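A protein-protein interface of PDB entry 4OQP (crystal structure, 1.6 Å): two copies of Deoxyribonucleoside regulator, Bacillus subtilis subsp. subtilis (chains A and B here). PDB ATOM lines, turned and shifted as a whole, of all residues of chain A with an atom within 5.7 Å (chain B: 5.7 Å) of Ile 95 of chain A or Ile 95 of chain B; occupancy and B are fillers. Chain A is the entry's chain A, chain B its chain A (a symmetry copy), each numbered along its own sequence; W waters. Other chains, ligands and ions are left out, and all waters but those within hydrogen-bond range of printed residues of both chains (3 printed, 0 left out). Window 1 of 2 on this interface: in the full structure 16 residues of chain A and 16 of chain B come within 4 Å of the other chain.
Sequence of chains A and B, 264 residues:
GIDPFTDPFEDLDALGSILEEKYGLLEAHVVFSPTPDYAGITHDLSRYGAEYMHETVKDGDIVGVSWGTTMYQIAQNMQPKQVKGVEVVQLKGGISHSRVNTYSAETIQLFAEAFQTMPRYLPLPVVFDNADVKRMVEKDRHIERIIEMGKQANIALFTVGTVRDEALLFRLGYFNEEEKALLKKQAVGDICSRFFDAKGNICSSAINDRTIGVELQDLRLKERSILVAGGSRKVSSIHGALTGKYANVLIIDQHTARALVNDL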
ATOM      1  N   GLN A  90     -19.676  -6.301   9.662  1.00  0.00           N
ATOM      2  CA  GLN A  90     -18.528  -6.429   8.830  1.00  0.00           C
ATOM      3  C   GLN A  90     -18.718  -5.592   7.551  1.00  0.00           C
ATOM      4  O   GLN A  90     -19.749  -5.737   6.879  1.00  0.00           O
ATOM      5  CB  GLN A  90     -18.378  -7.913   8.512  1.00  0.00           C
ATOM      6  CG  GLN A  90     -17.124  -8.299   7.834  1.00  0.00           C
ATOM      7  CD  GLN A  90     -16.934  -9.799   7.787  1.00  0.00           C
ATOM      8  OE1 GLN A  90     -17.636 -10.562   8.483  1.00  0.00           O
ATOM      9  NE2 GLN A  90     -16.006 -10.233   6.958  1.00  0.00           N
ATOM     10  N   GLY A  93     -16.598  -8.697   3.135  1.00  0.00           N
ATOM     11  CA  GLY A  93     -16.313 -10.130   3.428  1.00  0.00           C
ATOM     12  C   GLY A  93     -14.839 -10.414   3.495  1.00  0.00           C
ATOM     13  O   GLY A  93     -14.025  -9.689   2.929  1.00  0.00           O
ATOM     14  N   GLY A  94     -14.494 -11.456   4.245  1.00  0.00           N
ATOM     15  CA  GLY A  94     -13.123 -11.836   4.555  1.00  0.00           C
ATOM     16  C   GLY A  94     -12.804 -13.257   4.196  1.00  0.00           C
ATOM     17  O   GLY A  94     -11.747 -13.797   4.577  1.00  0.00           O
ATOM     18  N   ILE A  95     -13.660 -13.874   3.386  1.00  0.00           N
ATOM     19  CA  ILE A  95     -13.360 -15.232   2.949  1.00  0.00           C
ATOM     20  C   ILE A  95     -12.177 -15.237   1.981  1.00  0.00           C
ATOM     21  O   ILE A  95     -12.130 -14.461   1.019  1.00  0.00           O
ATOM     22  CB  ILE A  95     -14.584 -15.915   2.328  1.00  0.00           C
ATOM     23  CG1 ILE A  95     -15.677 -16.094   3.369  1.00  0.00           C
ATOM     24  CG2 ILE A  95     -14.154 -17.211   1.610  1.00  0.00           C
ATOM     25  CD1 ILE A  95     -16.907 -16.759   2.835  1.00  0.00           C
ATOM     26  N   SER A  96     -11.251 -16.134   2.245  1.00  0.00           N
ATOM     27  CA  SER A  96     -10.088 -16.414   1.402  1.00  0.00           C
ATOM     28  C   SER A  96     -10.295 -17.652   0.533  1.00  0.00           C
ATOM     29  O   SER A  96     -10.918 -18.621   0.969  1.00  0.00           O
ATOM     30  CB  SER A  96      -8.826 -16.627   2.266  1.00  0.00           C
ATOM     31  OG  SER A  96      -7.693 -16.971   1.466  1.00  0.00           O
ATOM     32  N   HIS A  97      -9.796 -17.616  -0.710  1.00  0.00           N
ATOM     33  CA  HIS A  97      -9.718 -18.785  -1.553  1.00  0.00           C
ATOM     34  C   HIS A  97      -8.323 -19.403  -1.582  1.00  0.00           C
ATOM     35  O   HIS A  97      -8.058 -20.332  -2.372  1.00  0.00           O
ATOM     36  CB  HIS A  97     -10.262 -18.452  -2.939  1.00  0.00           C
ATOM     37  CG  HIS A  97     -11.753 -18.450  -3.003  1.00  0.00           C
ATOM     38  ND1 HIS A  97     -12.435 -18.364  -4.187  1.00  0.00           N
ATOM     39  CD2 HIS A  97     -12.692 -18.434  -2.027  1.00  0.00           C
ATOM     40  CE1 HIS A  97     -13.740 -18.332  -3.948  1.00  0.00           C
ATOM     41  NE2 HIS A  97     -13.920 -18.382  -2.636  1.00  0.00           N
ATOM     42  N   THR A 102      -7.750 -14.352   6.796  1.00  0.00           N
ATOM     43  CA  THR A 102      -7.805 -12.941   7.094  1.00  0.00           C
ATOM     44  C   THR A 102      -8.096 -12.645   8.567  1.00  0.00           C
ATOM     45  O   THR A 102      -7.965 -11.497   8.995  1.00  0.00           O
ATOM     46  CB  THR A 102      -8.907 -12.221   6.289  1.00  0.00           C
ATOM     47  OG1 THR A 102     -10.186 -12.762   6.660  1.00  0.00           O
ATOM     48  CG2 THR A 102      -8.707 -12.353   4.831  1.00  0.00           C
ATOM     49  N   SER A 104     -10.931 -12.315   9.701  1.00  0.00           N
ATOM     50  CA  SER A 104     -12.005 -11.379   9.772  1.00  0.00           C
ATOM     51  C   SER A 104     -13.051 -11.743  10.790  1.00  0.00           C
ATOM     52  O   SER A 104     -13.606 -10.849  11.411  1.00  0.00           O
ATOM     53  CB  SER A 104     -12.635 -11.179   8.382  1.00  0.00           C
ATOM     54  OG  SER A 104     -13.320 -12.340   7.935  1.00  0.00           O
ATOM     55  N   LEU A 122     -20.447 -10.811   7.119  1.00  0.00           N
ATOM     56  CA  LEU A 122     -20.646 -10.705   5.682  1.00  0.00           C
ATOM     57  C   LEU A 122     -19.915 -11.949   5.128  1.00  0.00           C
ATOM     58  O   LEU A 122     -18.691 -11.925   4.927  1.00  0.00           O
ATOM     59  CB  LEU A 122     -20.080  -9.380   5.156  1.00  0.00           C
ATOM     60  CG  LEU A 122     -20.255  -9.090   3.661  1.00  0.00           C
ATOM     61  CD1 LEU A 122     -21.642  -9.483   3.191  1.00  0.00           C
ATOM     62  CD2 LEU A 122     -19.989  -7.606   3.424  1.00  0.00           C
ATOM     63  N   PRO A 123     -20.649 -13.060   4.947  1.00  0.00           N
ATOM     64  CA  PRO A 123     -20.009 -14.383   4.699  1.00  0.00           C
ATOM     65  C   PRO A 123     -19.684 -14.629   3.224  1.00  0.00           C
ATOM     66  O   PRO A 123     -20.251 -15.522   2.592  1.00  0.00           O
ATOM     67  CB  PRO A 123     -21.048 -15.351   5.209  1.00  0.00           C
ATOM     68  CG  PRO A 123     -22.366 -14.633   4.945  1.00  0.00           C
ATOM     69  CD  PRO A 123     -22.104 -13.199   5.187  1.00  0.00           C
ATOM     70  N   LEU A 124     -18.748 -13.820   2.733  1.00  0.00           N
ATOM     71  CA  LEU A 124     -18.396 -13.765   1.319  1.00  0.00           C
ATOM     72  C   LEU A 124     -16.901 -13.458   1.179  1.00  0.00           C
ATOM     73  O   LEU A 124     -16.305 -12.883   2.084  1.00  0.00           O
ATOM     74  CB  LEU A 124     -19.143 -12.645   0.655  1.00  0.00           C
ATOM     75  CG  LEU A 124     -20.653 -12.759   0.529  1.00  0.00           C
ATOM     76  CD1 LEU A 124     -21.132 -11.476  -0.135  1.00  0.00           C
ATOM     77  CD2 LEU A 124     -21.118 -13.924  -0.279  1.00  0.00           C
ATOM     78  N   PRO A 125     -16.327 -13.789   0.036  1.00  0.00           N
ATOM     79  CA  PRO A 125     -15.063 -13.103  -0.319  1.00  0.00           C
ATOM     80  C   PRO A 125     -15.363 -11.641  -0.645  1.00  0.00           C
ATOM     81  O   PRO A 125     -16.515 -11.293  -0.896  1.00  0.00           O
ATOM     82  CB  PRO A 125     -14.596 -13.848  -1.555  1.00  0.00           C
ATOM     83  CG  PRO A 125     -15.883 -14.290  -2.198  1.00  0.00           C
ATOM     84  CD  PRO A 125     -16.823 -14.627  -1.069  1.00  0.00           C
ATOM     85  N   VAL A 126     -14.354 -10.763  -0.624  1.00  0.00           N
ATOM     86  CA  VAL A 126     -14.613  -9.365  -0.947  1.00  0.00           C
ATOM     87  C   VAL A 126     -14.557  -9.160  -2.457  1.00  0.00           C
ATOM     88  O   VAL A 126     -15.278  -8.316  -2.969  1.00  0.00           O
ATOM     89  CB  VAL A 126     -13.747  -8.355  -0.132  1.00  0.00           C
ATOM     90  CG1 VAL A 126     -12.286  -8.663  -0.223  1.00  0.00           C
ATOM     91  CG2 VAL A 126     -14.032  -6.920  -0.523  1.00  0.00           C
ATOM     92  N   LEU A 172      -4.906 -14.005  -1.244  1.00  0.00           N
ATOM     93  CA  LEU A 172      -6.191 -14.627  -0.962  1.00  0.00           C
ATOM     94  C   LEU A 172      -6.828 -15.327  -2.178  1.00  0.00           C
ATOM     95  O   LEU A 172      -7.956 -15.826  -2.088  1.00  0.00           O
ATOM     96  CB  LEU A 172      -7.170 -13.579  -0.401  1.00  0.00           C
ATOM     97  CG  LEU A 172      -6.668 -12.799   0.787  1.00  0.00           C
ATOM     98  CD1 LEU A 172      -7.696 -11.788   1.251  1.00  0.00           C
ATOM     99  CD2 LEU A 172      -6.367 -13.718   1.954  1.00  0.00           C
ATOM    100  N   TYR A 174      -7.675 -13.964  -5.021  1.00  0.00           N
ATOM    101  CA  TYR A 174      -8.623 -13.075  -5.712  1.00  0.00           C
ATOM    102  C   TYR A 174      -8.137 -12.676  -7.097  1.00  0.00           C
ATOM    103  O   TYR A 174      -8.953 -12.513  -8.000  1.00  0.00           O
ATOM    104  CB  TYR A 174      -8.866 -11.791  -4.925  1.00  0.00           C
ATOM    105  CG  TYR A 174      -9.542 -11.958  -3.584  1.00  0.00           C
ATOM    106  CD1 TYR A 174     -10.309 -13.072  -3.254  1.00  0.00           C
ATOM    107  CD2 TYR A 174      -9.487 -10.937  -2.682  1.00  0.00           C
ATOM    108  CE1 TYR A 174     -10.919 -13.175  -2.008  1.00  0.00           C
ATOM    109  CE2 TYR A 174     -10.072 -11.016  -1.456  1.00  0.00           C
ATOM    110  CZ  TYR A 174     -10.836 -12.105  -1.111  1.00  0.00           C
ATOM    111  OH  TYR A 174     -11.465 -12.106   0.129  1.00  0.00           O
ATOM    112  N   GLN B  90     -14.189 -30.703   2.684  1.00  0.00           N
ATOM    113  CA  GLN B  90     -15.556 -30.480   3.009  1.00  0.00           C
ATOM    114  C   GLN B  90     -16.443 -30.849   1.804  1.00  0.00           C
ATOM    115  O   GLN B  90     -16.186 -30.368   0.692  1.00  0.00           O
ATOM    116  CB  GLN B  90     -15.687 -29.004   3.370  1.00  0.00           C
ATOM    117  CG  GLN B  90     -16.985 -28.599   3.948  1.00  0.00           C
ATOM    118  CD  GLN B  90     -16.949 -27.197   4.515  1.00  0.00           C
ATOM    119  OE1 GLN B  90     -15.868 -26.599   4.694  1.00  0.00           O
ATOM    120  NE2 GLN B  90     -18.122 -26.657   4.781  1.00  0.00           N
ATOM    121  N   GLY B  93     -20.627 -26.847   1.461  1.00  0.00           N
ATOM    122  CA  GLY B  93     -20.425 -25.626   2.291  1.00  0.00           C
ATOM    123  C   GLY B  93     -21.360 -25.576   3.466  1.00  0.00           C
ATOM    124  O   GLY B  93     -22.423 -26.193   3.461  1.00  0.00           O
ATOM    125  N   GLY B  94     -20.928 -24.871   4.508  1.00  0.00           N
ATOM    126  CA  GLY B  94     -21.608 -24.792   5.793  1.00  0.00           C
ATOM    127  C   GLY B  94     -21.893 -23.386   6.229  1.00  0.00           C
ATOM    128  O   GLY B  94     -22.283 -23.136   7.387  1.00  0.00           O
ATOM    129  N   ILE B  95     -21.792 -22.441   5.298  1.00  0.00           N
ATOM    130  CA  ILE B  95     -22.129 -21.067   5.652  1.00  0.00           C
ATOM    131  C   ILE B  95     -23.633 -20.922   5.878  1.00  0.00           C
ATOM    132  O   ILE B  95     -24.451 -21.363   5.061  1.00  0.00           O
ATOM    133  CB  ILE B  95     -21.629 -20.069   4.601  1.00  0.00           C
ATOM    134  CG1 ILE B  95     -20.111 -20.075   4.541  1.00  0.00           C
ATOM    135  CG2 ILE B  95     -22.263 -18.684   4.849  1.00  0.00           C
ATOM    136  CD1 ILE B  95     -19.548 -19.119   3.536  1.00  0.00           C
ATOM    137  N   SER B  96     -23.967 -20.283   6.978  1.00  0.00           N
ATOM    138  CA  SER B  96     -25.333 -19.914   7.353  1.00  0.00           C
ATOM    139  C   SER B  96     -25.640 -18.453   7.037  1.00  0.00           C
ATOM    140  O   SER B  96     -24.770 -17.591   7.171  1.00  0.00           O
ATOM    141  CB  SER B  96     -25.566 -20.148   8.862  1.00  0.00           C
ATOM    142  OG  SER B  96     -26.872 -19.729   9.263  1.00  0.00           O
ATOM    143  N   HIS B  97     -26.872 -18.170   6.590  1.00  0.00           N
ATOM    144  CA  HIS B  97     -27.368 -16.820   6.471  1.00  0.00           C
ATOM    145  C   HIS B  97     -28.272 -16.415   7.632  1.00  0.00           C
ATOM    146  O   HIS B  97     -28.891 -15.332   7.605  1.00  0.00           O
ATOM    147  CB  HIS B  97     -28.018 -16.634   5.104  1.00  0.00           C
ATOM    148  CG  HIS B  97     -27.031 -16.417   4.005  1.00  0.00           C
ATOM    149  ND1 HIS B  97     -27.409 -16.042   2.744  1.00  0.00           N
ATOM    150  CD2 HIS B  97     -25.691 -16.607   3.954  1.00  0.00           C
ATOM    151  CE1 HIS B  97     -26.340 -15.971   1.961  1.00  0.00           C
ATOM    152  NE2 HIS B  97     -25.279 -16.305   2.681  1.00  0.00           N
ATOM    153  N   THR B 102     -23.405 -23.830  11.799  1.00  0.00           N
ATOM    154  CA  THR B 102     -23.344 -25.244  11.515  1.00  0.00           C
ATOM    155  C   THR B 102     -22.138 -25.938  12.152  1.00  0.00           C
ATOM    156  O   THR B 102     -22.078 -27.168  12.162  1.00  0.00           O
ATOM    157  CB  THR B 102     -23.248 -25.526  10.000  1.00  0.00           C
ATOM    158  OG1 THR B 102     -22.027 -24.961   9.496  1.00  0.00           O
ATOM    159  CG2 THR B 102     -24.401 -24.980   9.258  1.00  0.00           C
ATOM    160  N   SER B 104     -19.414 -26.219  10.759  1.00  0.00           N
ATOM    161  CA  SER B 104     -18.745 -26.979   9.755  1.00  0.00           C
ATOM    162  C   SER B 104     -17.250 -26.810   9.772  1.00  0.00           C
ATOM    163  O   SER B 104     -16.545 -27.770   9.497  1.00  0.00           O
ATOM    164  CB  SER B 104     -19.321 -26.655   8.365  1.00  0.00           C
ATOM    165  OG  SER B 104     -19.008 -25.332   7.953  1.00  0.00           O
ATOM    166  N   LEU B 122     -14.854 -25.569   1.912  1.00  0.00           N
ATOM    167  CA  LEU B 122     -15.749 -25.200   0.827  1.00  0.00           C
ATOM    168  C   LEU B 122     -16.482 -23.955   1.376  1.00  0.00           C
ATOM    169  O   LEU B 122     -17.475 -24.079   2.110  1.00  0.00           O
ATOM    170  CB  LEU B 122     -16.691 -26.361   0.487  1.00  0.00           C
ATOM    171  CG  LEU B 122     -17.669 -26.151  -0.676  1.00  0.00           C
ATOM    172  CD1 LEU B 122     -16.989 -25.450  -1.836  1.00  0.00           C
ATOM    173  CD2 LEU B 122     -18.219 -27.511  -1.095  1.00  0.00           C
ATOM    174  N   PRO B 123     -15.954 -22.754   1.084  1.00  0.00           N
ATOM    175  CA  PRO B 123     -16.396 -21.517   1.788  1.00  0.00           C
ATOM    176  C   PRO B 123     -17.634 -20.875   1.159  1.00  0.00           C
ATOM    177  O   PRO B 123     -17.570 -19.764   0.630  1.00  0.00           O
ATOM    178  CB  PRO B 123     -15.186 -20.624   1.673  1.00  0.00           C
ATOM    179  CG  PRO B 123     -14.556 -21.043   0.351  1.00  0.00           C
ATOM    180  CD  PRO B 123     -14.757 -22.503   0.248  1.00  0.00           C
ATOM    181  N   LEU B 124     -18.738 -21.611   1.261  1.00  0.00           N
ATOM    182  CA  LEU B 124     -19.992 -21.274   0.596  1.00  0.00           C
ATOM    183  C   LEU B 124     -21.168 -21.719   1.472  1.00  0.00           C
ATOM    184  O   LEU B 124     -21.016 -22.619   2.292  1.00  0.00           O
ATOM    185  CB  LEU B 124     -20.095 -22.024  -0.700  1.00  0.00           C
ATOM    186  CG  LEU B 124     -19.123 -21.677  -1.815  1.00  0.00           C
ATOM    187  CD1 LEU B 124     -19.433 -22.617  -2.971  1.00  0.00           C
ATOM    188  CD2 LEU B 124     -19.219 -20.268  -2.299  1.00  0.00           C
ATOM    189  N   PRO B 125     -22.331 -21.133   1.257  1.00  0.00           N
ATOM    190  CA  PRO B 125     -23.550 -21.838   1.715  1.00  0.00           C
ATOM    191  C   PRO B 125     -23.768 -23.075   0.846  1.00  0.00           C
ATOM    192  O   PRO B 125     -23.195 -23.172  -0.238  1.00  0.00           O
ATOM    193  CB  PRO B 125     -24.650 -20.818   1.492  1.00  0.00           C
ATOM    194  CG  PRO B 125     -24.156 -20.031   0.307  1.00  0.00           C
ATOM    195  CD  PRO B 125     -22.659 -19.937   0.461  1.00  0.00           C
ATOM    196  N   VAL B 126     -24.570 -24.043   1.304  1.00  0.00           N
ATOM    197  CA  VAL B 126     -24.806 -25.226   0.484  1.00  0.00           C
ATOM    198  C   VAL B 126     -25.943 -24.961  -0.497  1.00  0.00           C
ATOM    199  O   VAL B 126     -25.919 -25.502  -1.594  1.00  0.00           O
ATOM    200  CB  VAL B 126     -24.963 -26.544   1.304  1.00  0.00           C
ATOM    201  CG1 VAL B 126     -25.998 -26.421   2.377  1.00  0.00           C
ATOM    202  CG2 VAL B 126     -25.234 -27.737   0.411  1.00  0.00           C
ATOM    203  N   LEU B 172     -31.119 -22.061   8.606  1.00  0.00           N
ATOM    204  CA  LEU B 172     -29.946 -21.390   8.066  1.00  0.00           C
ATOM    205  C   LEU B 172     -30.274 -20.270   7.058  1.00  0.00           C
ATOM    206  O   LEU B 172     -29.363 -19.677   6.470  1.00  0.00           O
ATOM    207  CB  LEU B 172     -29.011 -22.419   7.404  1.00  0.00           C
ATOM    208  CG  LEU B 172     -28.621 -23.587   8.275  1.00  0.00           C
ATOM    209  CD1 LEU B 172     -27.714 -24.544   7.529  1.00  0.00           C
ATOM    210  CD2 LEU B 172     -27.879 -23.120   9.511  1.00  0.00           C
ATOM    211  N   TYR B 174     -31.885 -20.566   4.234  1.00  0.00           N
ATOM    212  CA  TYR B 174     -31.837 -21.064   2.850  1.00  0.00           C
ATOM    213  C   TYR B 174     -33.209 -21.078   2.192  1.00  0.00           C
ATOM    214  O   TYR B 174     -33.305 -20.845   0.990  1.00  0.00           O
ATOM    215  CB  TYR B 174     -31.282 -22.483   2.781  1.00  0.00           C
ATOM    216  CG  TYR B 174     -29.841 -22.648   3.204  1.00  0.00           C
ATOM    217  CD1 TYR B 174     -28.927 -21.599   3.213  1.00  0.00           C
ATOM    218  CD2 TYR B 174     -29.376 -23.896   3.501  1.00  0.00           C
ATOM    219  CE1 TYR B 174     -27.608 -21.804   3.603  1.00  0.00           C
ATOM    220  CE2 TYR B 174     -28.091 -24.120   3.888  1.00  0.00           C
ATOM    221  CZ  TYR B 174     -27.172 -23.099   3.901  1.00  0.00           C
ATOM    222  OH  TYR B 174     -25.858 -23.396   4.243  1.00  0.00           O
HETATM  223  O   HOH W   1     -22.754 -16.497   1.553  1.00  0.00           O
HETATM  224  O   HOH W   2     -19.401 -17.430   0.481  1.00  0.00           O
HETATM  225  O   HOH W   3     -16.442 -18.190  -1.503  1.00  0.00           O
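Water W3 lies within hydrogen-bond range of NE2 of His 97 of chain A (2.8 Å) and O of Pro 123 of chain B (2.9 Å).
Water W1 lies within hydrogen-bond range of a ring nitrogen (NE2) of His 97 of chain B (2.8 Å) and the backbone carbonyl oxygen (O) of Pro 123 of chain A (2.9 Å).
Water W2 bridges the backbone carbonyl oxygen of Pro 123 of chain A and the backbone carbonyl oxygen of Pro 123 of chain B.
Ile 95 of chain A touches just these residues of chain B: Ile 95 and Pro 123.
Ile 95 of chain B touches just these residues of chain A: Ile 95 and Pro 123.
Of the printed residues of chain B, His 97 of chain A touches Pro 123 (3.99 Å).
Of the printed residues of chain A, His 97 of chain B touches Pro 123 (3.99 Å).
The nearest residue of chain B that does not touch Ile 95 of chain A is Leu 124 of chain B (5.4 Å).
The nearest printed residue of chain B that does not touch His 97 of chain A is Leu 124 of chain B (5.6 Å).
The backbone NH (N) of Ile 95 of chain A sits at hydrogen-bond distance from the backbone carbonyl oxygen (O) of Leu 124 of chain A (3.1 Å).
The side-chain hydroxyl (OH) of Tyr 174 of chain A sits at hydrogen-bond distance from the backbone carbonyl oxygen (O) of Ile 95 of chain A (2.6 Å).
The backbone carbonyl oxygen of Leu 172 of chain A is in hydrogen-bond range of the backbone NH of His 97 of chain A (2.9 Å).
N of Ile 95 of chain B sits at hydrogen-bond distance from O of Leu 124 of chain B (3.1 Å).
The side-chain hydroxyl (OH) of Tyr 174 of chain B is in hydrogen-bond range of the backbone carbonyl oxygen (O) of Ile 95 of chain B.
The backbone carbonyl oxygen (O) of Leu 172 of chain B sits at hydrogen-bond distance from the backbone NH (N) of His 97 of chain B, 2.9 Å away.
Ile 95 of chain A touches its own counterpart, Ile 95 of chain B.
Ile 95 of chain A touches Pro 123 of chain B, and with the chains exchanged Pro 123 of chain A touches Ile 95 of chain B.
His 97 of chain A touches Pro 123 of chain B, and with the chains exchanged Pro 123 of chain A touches His 97 of chain B.
Positions printed for both chains: 90, 93, 94, 95, 96, 97, 102, 104, 122, 123, 124, 125, 126, 172 and 174.
Of the 5 pairs that touch across the chains among the printed residues, 5 have their exchanged pair printed and touching as well.
Among the printed residues, merely in contact across the chains: Ile 95 of chain A with Ile 95 of chain B, Ile 95 of chain A with Pro 123 of chain B, His 97 of chain A with Pro 123 of chain B, Pro 123 of chain A with Ile 95 of chain B and Pro 123 of chain A with His 97 of chain B.
Of the 15 printed residues of chain B, 3 touch a printed residue of chain A.
Printed residues of chain B that touch a printed residue of chain A: Ile 95, His 97 and Pro 123.
Hydrophobic or aromatic side chains of chain B within 4 Å of the printed part of chain A: Ile 95, His 97 and Pro 123.
Along chain B the printed residues that touch a printed residue of chain A span positions 95 to 123.
Of the 15 printed residues of chain A, 3 touch a printed residue of chain B.
Printed residues of chain A that touch a printed residue of chain B: Ile 95, His 97 and Pro 123.
Hydrophobic or aromatic side chains of chain A that line the printed part of chain B: Ile 95, His 97 and Pro 123.
Along chain A the printed residues that touch a printed residue of chain B span positions 95 to 123.
Among the printed residues, 5 pairs touch across the chains.
Among the printed residues, no Asp or Glu carboxylate lies within 4 Å of a Lys or Arg side-chain nitrogen of the other chain.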
